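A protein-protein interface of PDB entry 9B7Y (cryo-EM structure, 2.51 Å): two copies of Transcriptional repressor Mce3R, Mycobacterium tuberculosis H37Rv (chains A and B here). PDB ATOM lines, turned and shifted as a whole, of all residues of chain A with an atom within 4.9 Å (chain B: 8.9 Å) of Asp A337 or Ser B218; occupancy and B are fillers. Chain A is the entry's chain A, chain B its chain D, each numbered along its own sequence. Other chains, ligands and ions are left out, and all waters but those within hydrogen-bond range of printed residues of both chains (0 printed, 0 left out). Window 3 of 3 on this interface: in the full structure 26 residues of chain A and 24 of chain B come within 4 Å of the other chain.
The guanidinium group (NH1) of Arg A333 is in hydrogen-bond range of the side-chain amide oxygen (OD1) of Asn A334 (2.8 Å).
The side-chain hydroxyl of Ser B218 lies close to the backbone NH of Glu B221 (3.3 Å).
O of Ser B218 is in hydrogen-bond range of OG1 of Thr B222 (2.9 Å).
CD1 of Tyr B220 touches NH1 of Arg A333, 3.5 Å away.
NH2 of Arg A333 touches O of Ser B258, at 3.8 Å.
Asn A334 touches Tyr B220 (OD1 to CD2, 3.97 Å).
OD2 of Asp A337 touches CB of Ser B218, 3.4 Å away.
Val A341 touches Phe B217 (CG2 to CB, 3.6 Å).
Of chain B, only Ser B218 comes within 4 Å of Asp A337.
Ser B218 touches just one residue of chain A: Asp A337.
No residue of chain B comes within 4 Å of Gly A336.
Of the printed residues of chain A, Ser B258 touches Arg A333.
Printed residues of chain B within 4 Å of Asn A334: Tyr B220 (3.97 Å).
Of the printed residues of chain B, Arg A333 touches Tyr B220 and Ser B258.
Printed residues of chain A within 4 Å of Phe B217: Val A341 (3.6 Å).
Printed residues of chain B within 4 Å of Val A341: Phe B217 (3.6 Å).
Arg B272 touches none of the printed residues of chain A.
Of the 9 printed residues of chain A, 4 touch a printed residue of chain B.
Printed residues of chain A that touch a printed residue of chain B: Arg A333, Asn A334, Asp A337 and Val A341.
Along chain A the printed residues that touch a printed residue of chain B span positions 333 to 341.
Of the 18 printed residues of chain B, 4 touch a printed residue of chain A.
Printed residues of chain B that touch a printed residue of chain A: Phe B217, Ser B218, Tyr B220 and Ser B258.
Hydrophobic or aromatic side chains of chain B within 4 Å of the printed part of chain A: Phe B217 and Tyr B220.
No position is printed for both chains.
Of the 5 pairs that touch across the chains among the printed residues, none has its exchanged pair printed and touching as well.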
ATOM      1  N   ARG A 333      18.102  17.858 -35.664  1.00  0.00           N
ATOM      2  CA  ARG A 333      17.868  18.954 -34.729  1.00  0.00           C
ATOM      3  C   ARG A 333      17.276  18.453 -33.415  1.00  0.00           C
ATOM      4  O   ARG A 333      17.697  18.880 -32.332  1.00  0.00           O
ATOM      5  CB  ARG A 333      16.956  19.997 -35.374  1.00  0.00           C
ATOM      6  CG  ARG A 333      16.933  21.341 -34.665  1.00  0.00           C
ATOM      7  CD  ARG A 333      15.505  21.764 -34.369  1.00  0.00           C
ATOM      8  NE  ARG A 333      14.705  21.839 -35.584  1.00  0.00           N
ATOM      9  CZ  ARG A 333      13.634  21.096 -35.825  1.00  0.00           C
ATOM     10  NH1 ARG A 333      13.205  20.199 -34.952  1.00  0.00           N
ATOM     11  NH2 ARG A 333      12.979  21.254 -36.972  1.00  0.00           N
ATOM     12  N   ASN A 334      16.295  17.548 -33.485  1.00  0.00           N
ATOM     13  CA  ASN A 334      15.706  17.010 -32.262  1.00  0.00           C
ATOM     14  C   ASN A 334      16.726  16.203 -31.464  1.00  0.00           C
ATOM     15  O   ASN A 334      16.787  16.309 -30.228  1.00  0.00           O
ATOM     16  CB  ASN A 334      14.486  16.154 -32.600  1.00  0.00           C
ATOM     17  CG  ASN A 334      13.400  16.941 -33.309  1.00  0.00           C
ATOM     18  OD1 ASN A 334      13.228  18.135 -33.072  1.00  0.00           O
ATOM     19  ND2 ASN A 334      12.662  16.273 -34.186  1.00  0.00           N
ATOM     20  N   GLN A 335      17.534  15.392 -32.152  1.00  0.00           N
ATOM     21  CA  GLN A 335      18.580  14.640 -31.467  1.00  0.00           C
ATOM     22  C   GLN A 335      19.582  15.578 -30.810  1.00  0.00           C
ATOM     23  O   GLN A 335      20.038  15.324 -29.690  1.00  0.00           O
ATOM     24  CB  GLN A 335      19.277  13.700 -32.451  1.00  0.00           C
ATOM     25  CG  GLN A 335      19.819  12.428 -31.820  1.00  0.00           C
ATOM     26  CD  GLN A 335      18.795  11.723 -30.952  1.00  0.00           C
ATOM     27  OE1 GLN A 335      17.691  11.419 -31.400  1.00  0.00           O
ATOM     28  NE2 GLN A 335      19.158  11.463 -29.703  1.00  0.00           N
ATOM     29  N   GLY A 336      19.933  16.671 -31.491  1.00  0.00           N
ATOM     30  CA  GLY A 336      20.835  17.644 -30.901  1.00  0.00           C
ATOM     31  C   GLY A 336      20.254  18.314 -29.673  1.00  0.00           C
ATOM     32  O   GLY A 336      20.964  18.566 -28.701  1.00  0.00           O
ATOM     33  N   ASP A 337      18.954  18.617 -29.700  1.00  0.00           N
ATOM     34  CA  ASP A 337      18.315  19.223 -28.533  1.00  0.00           C
ATOM     35  C   ASP A 337      18.324  18.270 -27.340  1.00  0.00           C
ATOM     36  O   ASP A 337      18.643  18.665 -26.209  1.00  0.00           O
ATOM     37  CB  ASP A 337      16.885  19.642 -28.881  1.00  0.00           C
ATOM     38  CG  ASP A 337      16.839  20.765 -29.900  1.00  0.00           C
ATOM     39  OD1 ASP A 337      17.824  21.527 -29.991  1.00  0.00           O
ATOM     40  OD2 ASP A 337      15.818  20.888 -30.609  1.00  0.00           O
ATOM     41  N   ARG A 338      17.980  17.001 -27.578  1.00  0.00           N
ATOM     42  CA  ARG A 338      18.006  16.028 -26.487  1.00  0.00           C
ATOM     43  C   ARG A 338      19.425  15.825 -25.963  1.00  0.00           C
ATOM     44  O   ARG A 338      19.641  15.718 -24.746  1.00  0.00           O
ATOM     45  CB  ARG A 338      17.391  14.706 -26.947  1.00  0.00           C
ATOM     46  CG  ARG A 338      15.916  14.820 -27.307  1.00  0.00           C
ATOM     47  CD  ARG A 338      15.262  13.458 -27.470  1.00  0.00           C
ATOM     48  NE  ARG A 338      15.694  12.786 -28.689  1.00  0.00           N
ATOM     49  CZ  ARG A 338      15.049  12.847 -29.846  1.00  0.00           C
ATOM     50  NH1 ARG A 338      13.941  13.556 -29.983  1.00  0.00           N
ATOM     51  NH2 ARG A 338      15.530  12.184 -30.894  1.00  0.00           N
ATOM     52  N   GLU A 339      20.409  15.785 -26.862  1.00  0.00           N
ATOM     53  CA  GLU A 339      21.796  15.672 -26.431  1.00  0.00           C
ATOM     54  C   GLU A 339      22.245  16.903 -25.656  1.00  0.00           C
ATOM     55  O   GLU A 339      23.061  16.787 -24.739  1.00  0.00           O
ATOM     56  CB  GLU A 339      22.701  15.436 -27.639  1.00  0.00           C
ATOM     57  CG  GLU A 339      22.781  13.980 -28.065  1.00  0.00           C
ATOM     58  CD  GLU A 339      23.036  13.812 -29.548  1.00  0.00           C
ATOM     59  OE1 GLU A 339      23.754  14.652 -30.129  1.00  0.00           O
ATOM     60  OE2 GLU A 339      22.529  12.831 -30.130  1.00  0.00           O
ATOM     61  N   ALA A 340      21.734  18.084 -26.006  1.00  0.00           N
ATOM     62  CA  ALA A 340      22.041  19.284 -25.237  1.00  0.00           C
ATOM     63  C   ALA A 340      21.470  19.193 -23.829  1.00  0.00           C
ATOM     64  O   ALA A 340      22.104  19.635 -22.864  1.00  0.00           O
ATOM     65  CB  ALA A 340      21.506  20.522 -25.955  1.00  0.00           C
ATOM     66  N   VAL A 341      20.266  18.634 -23.695  1.00  0.00           N
ATOM     67  CA  VAL A 341      19.716  18.387 -22.362  1.00  0.00           C
ATOM     68  C   VAL A 341      20.627  17.445 -21.580  1.00  0.00           C
ATOM     69  O   VAL A 341      20.925  17.672 -20.396  1.00  0.00           O
ATOM     70  CB  VAL A 341      18.283  17.833 -22.467  1.00  0.00           C
ATOM     71  CG1 VAL A 341      17.773  17.405 -21.099  1.00  0.00           C
ATOM     72  CG2 VAL A 341      17.363  18.866 -23.086  1.00  0.00           C
ATOM     73  N   ALA B 213       6.740  22.998 -17.802  1.00  0.00           N
ATOM     74  CA  ALA B 213       7.746  23.942 -18.276  1.00  0.00           C
ATOM     75  C   ALA B 213       9.069  23.273 -18.634  1.00  0.00           C
ATOM     76  O   ALA B 213       9.716  23.670 -19.608  1.00  0.00           O
ATOM     77  CB  ALA B 213       7.985  25.025 -17.223  1.00  0.00           C
ATOM     78  N   ASP B 214       9.489  22.267 -17.863  1.00  0.00           N
ATOM     79  CA  ASP B 214      10.787  21.647 -18.111  1.00  0.00           C
ATOM     80  C   ASP B 214      10.759  20.751 -19.341  1.00  0.00           C
ATOM     81  O   ASP B 214      11.796  20.547 -19.982  1.00  0.00           O
ATOM     82  CB  ASP B 214      11.233  20.854 -16.885  1.00  0.00           C
ATOM     83  CG  ASP B 214      10.152  19.935 -16.364  1.00  0.00           C
ATOM     84  OD1 ASP B 214       9.048  19.933 -16.945  1.00  0.00           O
ATOM     85  OD2 ASP B 214      10.407  19.204 -15.385  1.00  0.00           O
ATOM     86  N   VAL B 215       9.589  20.205 -19.687  1.00  0.00           N
ATOM     87  CA  VAL B 215       9.489  19.354 -20.865  1.00  0.00           C
ATOM     88  C   VAL B 215       9.625  20.156 -22.150  1.00  0.00           C
ATOM     89  O   VAL B 215       9.801  19.571 -23.226  1.00  0.00           O
ATOM     90  CB  VAL B 215       8.166  18.568 -20.858  1.00  0.00           C
ATOM     91  CG1 VAL B 215       8.107  17.642 -19.653  1.00  0.00           C
ATOM     92  CG2 VAL B 215       6.983  19.520 -20.873  1.00  0.00           C
ATOM     93  N   LEU B 216       9.540  21.484 -22.073  1.00  0.00           N
ATOM     94  CA  LEU B 216       9.767  22.350 -23.229  1.00  0.00           C
ATOM     95  C   LEU B 216      11.243  22.739 -23.237  1.00  0.00           C
ATOM     96  O   LEU B 216      11.637  23.849 -22.869  1.00  0.00           O
ATOM     97  CB  LEU B 216       8.852  23.567 -23.180  1.00  0.00           C
ATOM     98  CG  LEU B 216       7.377  23.291 -22.879  1.00  0.00           C
ATOM     99  CD1 LEU B 216       6.569  24.576 -22.906  1.00  0.00           C
ATOM    100  CD2 LEU B 216       6.808  22.281 -23.862  1.00  0.00           C
ATOM    101  N   PHE B 217      12.073  21.794 -23.671  1.00  0.00           N
ATOM    102  CA  PHE B 217      13.522  21.922 -23.601  1.00  0.00           C
ATOM    103  C   PHE B 217      14.130  22.520 -24.864  1.00  0.00           C
ATOM    104  O   PHE B 217      15.358  22.575 -24.979  1.00  0.00           O
ATOM    105  CB  PHE B 217      14.159  20.561 -23.309  1.00  0.00           C
ATOM    106  CG  PHE B 217      13.673  19.455 -24.205  1.00  0.00           C
ATOM    107  CD1 PHE B 217      14.200  19.286 -25.475  1.00  0.00           C
ATOM    108  CD2 PHE B 217      12.695  18.577 -23.772  1.00  0.00           C
ATOM    109  CE1 PHE B 217      13.755  18.269 -26.296  1.00  0.00           C
ATOM    110  CE2 PHE B 217      12.248  17.558 -24.589  1.00  0.00           C
ATOM    111  CZ  PHE B 217      12.779  17.404 -25.851  1.00  0.00           C
ATOM    112  N   SER B 218      13.308  22.964 -25.810  1.00  0.00           N
ATOM    113  CA  SER B 218      13.819  23.537 -27.044  1.00  0.00           C
ATOM    114  C   SER B 218      12.787  24.499 -27.613  1.00  0.00           C
ATOM    115  O   SER B 218      11.620  24.503 -27.214  1.00  0.00           O
ATOM    116  CB  SER B 218      14.168  22.448 -28.065  1.00  0.00           C
ATOM    117  OG  SER B 218      13.009  21.744 -28.474  1.00  0.00           O
ATOM    118  N   ARG B 219      13.241  25.327 -28.556  1.00  0.00           N
ATOM    119  CA  ARG B 219      12.341  26.257 -29.228  1.00  0.00           C
ATOM    120  C   ARG B 219      11.263  25.510 -30.002  1.00  0.00           C
ATOM    121  O   ARG B 219      10.101  25.933 -30.034  1.00  0.00           O
ATOM    122  CB  ARG B 219      13.142  27.171 -30.156  1.00  0.00           C
ATOM    123  CG  ARG B 219      12.320  27.884 -31.213  1.00  0.00           C
ATOM    124  CD  ARG B 219      11.523  29.024 -30.609  1.00  0.00           C
ATOM    125  NE  ARG B 219      12.365  29.917 -29.822  1.00  0.00           N
ATOM    126  CZ  ARG B 219      13.148  30.857 -30.335  1.00  0.00           C
ATOM    127  NH1 ARG B 219      13.225  31.058 -31.639  1.00  0.00           N
ATOM    128  NH2 ARG B 219      13.872  31.615 -29.516  1.00  0.00           N
ATOM    129  N   TYR B 220      11.633  24.394 -30.634  1.00  0.00           N
ATOM    130  CA  TYR B 220      10.666  23.589 -31.373  1.00  0.00           C
ATOM    131  C   TYR B 220       9.568  23.067 -30.454  1.00  0.00           C
ATOM    132  O   TYR B 220       8.378  23.135 -30.785  1.00  0.00           O
ATOM    133  CB  TYR B 220      11.392  22.436 -32.068  1.00  0.00           C
ATOM    134  CG  TYR B 220      10.513  21.540 -32.909  1.00  0.00           C
ATOM    135  CD1 TYR B 220      10.206  21.871 -34.222  1.00  0.00           C
ATOM    136  CD2 TYR B 220      10.005  20.354 -32.395  1.00  0.00           C
ATOM    137  CE1 TYR B 220       9.409  21.051 -34.995  1.00  0.00           C
ATOM    138  CE2 TYR B 220       9.206  19.528 -33.160  1.00  0.00           C
ATOM    139  CZ  TYR B 220       8.912  19.882 -34.460  1.00  0.00           C
ATOM    140  OH  TYR B 220       8.117  19.062 -35.227  1.00  0.00           O
ATOM    141  N   GLU B 221       9.951  22.548 -29.284  1.00  0.00           N
ATOM    142  CA  GLU B 221       8.964  22.029 -28.341  1.00  0.00           C
ATOM    143  C   GLU B 221       8.059  23.136 -27.815  1.00  0.00           C
ATOM    144  O   GLU B 221       6.847  22.938 -27.672  1.00  0.00           O
ATOM    145  CB  GLU B 221       9.666  21.315 -27.186  1.00  0.00           C
ATOM    146  CG  GLU B 221      10.387  20.043 -27.592  1.00  0.00           C
ATOM    147  CD  GLU B 221       9.432  18.912 -27.913  1.00  0.00           C
ATOM    148  OE1 GLU B 221       8.608  18.565 -27.041  1.00  0.00           O
ATOM    149  OE2 GLU B 221       9.501  18.373 -29.037  1.00  0.00           O
ATOM    150  N   THR B 222       8.632  24.302 -27.509  1.00  0.00           N
ATOM    151  CA  THR B 222       7.826  25.421 -27.028  1.00  0.00           C
ATOM    152  C   THR B 222       6.828  25.873 -28.086  1.00  0.00           C
ATOM    153  O   THR B 222       5.654  26.115 -27.780  1.00  0.00           O
ATOM    154  CB  THR B 222       8.731  26.581 -26.614  1.00  0.00           C
ATOM    155  OG1 THR B 222       9.725  26.110 -25.695  1.00  0.00           O
ATOM    156  CG2 THR B 222       7.919  27.680 -25.946  1.00  0.00           C
ATOM    157  N   LEU B 223       7.277  25.985 -29.339  1.00  0.00           N
ATOM    158  CA  LEU B 223       6.370  26.357 -30.420  1.00  0.00           C
ATOM    159  C   LEU B 223       5.270  25.319 -30.598  1.00  0.00           C
ATOM    160  O   LEU B 223       4.102  25.672 -30.791  1.00  0.00           O
ATOM    161  CB  LEU B 223       7.149  26.542 -31.721  1.00  0.00           C
ATOM    162  CG  LEU B 223       7.858  27.880 -31.930  1.00  0.00           C
ATOM    163  CD1 LEU B 223       8.914  27.763 -33.013  1.00  0.00           C
ATOM    164  CD2 LEU B 223       6.848  28.952 -32.296  1.00  0.00           C
ATOM    165  N   LEU B 224       5.623  24.033 -30.531  1.00  0.00           N
ATOM    166  CA  LEU B 224       4.624  22.982 -30.688  1.00  0.00           C
ATOM    167  C   LEU B 224       3.581  23.035 -29.577  1.00  0.00           C
ATOM    168  O   LEU B 224       2.376  22.939 -29.841  1.00  0.00           O
ATOM    169  CB  LEU B 224       5.308  21.616 -30.718  1.00  0.00           C
ATOM    170  CG  LEU B 224       4.799  20.597 -31.737  1.00  0.00           C
ATOM    171  CD1 LEU B 224       4.976  21.118 -33.152  1.00  0.00           C
ATOM    172  CD2 LEU B 224       5.512  19.267 -31.563  1.00  0.00           C
ATOM    173  N   ALA B 225       4.027  23.199 -28.329  1.00  0.00           N
ATOM    174  CA  ALA B 225       3.091  23.260 -27.211  1.00  0.00           C
ATOM    175  C   ALA B 225       2.191  24.484 -27.304  1.00  0.00           C
ATOM    176  O   ALA B 225       0.977  24.387 -27.080  1.00  0.00           O
ATOM    177  CB  ALA B 225       3.856  23.255 -25.888  1.00  0.00           C
ATOM    178  N   GLY B 247       3.732  33.015 -27.559  1.00  0.00           N
ATOM    179  CA  GLY B 247       3.830  31.877 -26.661  1.00  0.00           C
ATOM    180  C   GLY B 247       5.234  31.308 -26.608  1.00  0.00           C
ATOM    181  O   GLY B 247       5.693  30.858 -25.555  1.00  0.00           O
ATOM    182  N   ALA B 248       5.934  31.318 -27.741  1.00  0.00           N
ATOM    183  CA  ALA B 248       7.340  30.936 -27.760  1.00  0.00           C
ATOM    184  C   ALA B 248       8.264  32.062 -27.319  1.00  0.00           C
ATOM    185  O   ALA B 248       9.453  31.812 -27.095  1.00  0.00           O
ATOM    186  CB  ALA B 248       7.743  30.466 -29.158  1.00  0.00           C
ATOM    187  N   SER B 258      11.752  27.571 -37.582  1.00  0.00           N
ATOM    188  CA  SER B 258      11.591  26.204 -37.107  1.00  0.00           C
ATOM    189  C   SER B 258      10.574  25.396 -37.897  1.00  0.00           C
ATOM    190  O   SER B 258      10.671  24.168 -37.918  1.00  0.00           O
ATOM    191  CB  SER B 258      11.184  26.197 -35.625  1.00  0.00           C
ATOM    192  OG  SER B 258      12.159  26.842 -34.825  1.00  0.00           O
ATOM    193  N   PHE B 259       9.607  26.044 -38.544  1.00  0.00           N
ATOM    194  CA  PHE B 259       8.564  25.358 -39.290  1.00  0.00           C
ATOM    195  C   PHE B 259       8.473  25.927 -40.698  1.00  0.00           C
ATOM    196  O   PHE B 259       8.795  27.093 -40.937  1.00  0.00           O
ATOM    197  CB  PHE B 259       7.198  25.480 -38.598  1.00  0.00           C
ATOM    198  CG  PHE B 259       7.133  24.806 -37.259  1.00  0.00           C
ATOM    199  CD1 PHE B 259       7.472  25.493 -36.106  1.00  0.00           C
ATOM    200  CD2 PHE B 259       6.729  23.486 -37.151  1.00  0.00           C
ATOM    201  CE1 PHE B 259       7.412  24.876 -34.871  1.00  0.00           C
ATOM    202  CE2 PHE B 259       6.666  22.865 -35.920  1.00  0.00           C
ATOM    203  CZ  PHE B 259       7.009  23.561 -34.780  1.00  0.00           C
ATOM    204  N   ARG B 272       2.830  13.183 -34.289  1.00  0.00           N
ATOM    205  CA  ARG B 272       3.308  12.817 -32.961  1.00  0.00           C
ATOM    206  C   ARG B 272       2.279  11.967 -32.227  1.00  0.00           C
ATOM    207  O   ARG B 272       2.616  10.932 -31.637  1.00  0.00           O
ATOM    208  CB  ARG B 272       3.635  14.080 -32.162  1.00  0.00           C
ATOM    209  CG  ARG B 272       3.875  13.842 -30.683  1.00  0.00           C
ATOM    210  CD  ARG B 272       4.310  15.121 -29.989  1.00  0.00           C
ATOM    211  NE  ARG B 272       5.572  15.623 -30.517  1.00  0.00           N
ATOM    212  CZ  ARG B 272       6.487  16.255 -29.796  1.00  0.00           C
ATOM    213  NH1 ARG B 272       6.313  16.487 -28.506  1.00  0.00           N
ATOM    214  NH2 ARG B 272       7.606  16.667 -30.386  1.00  0.00           N
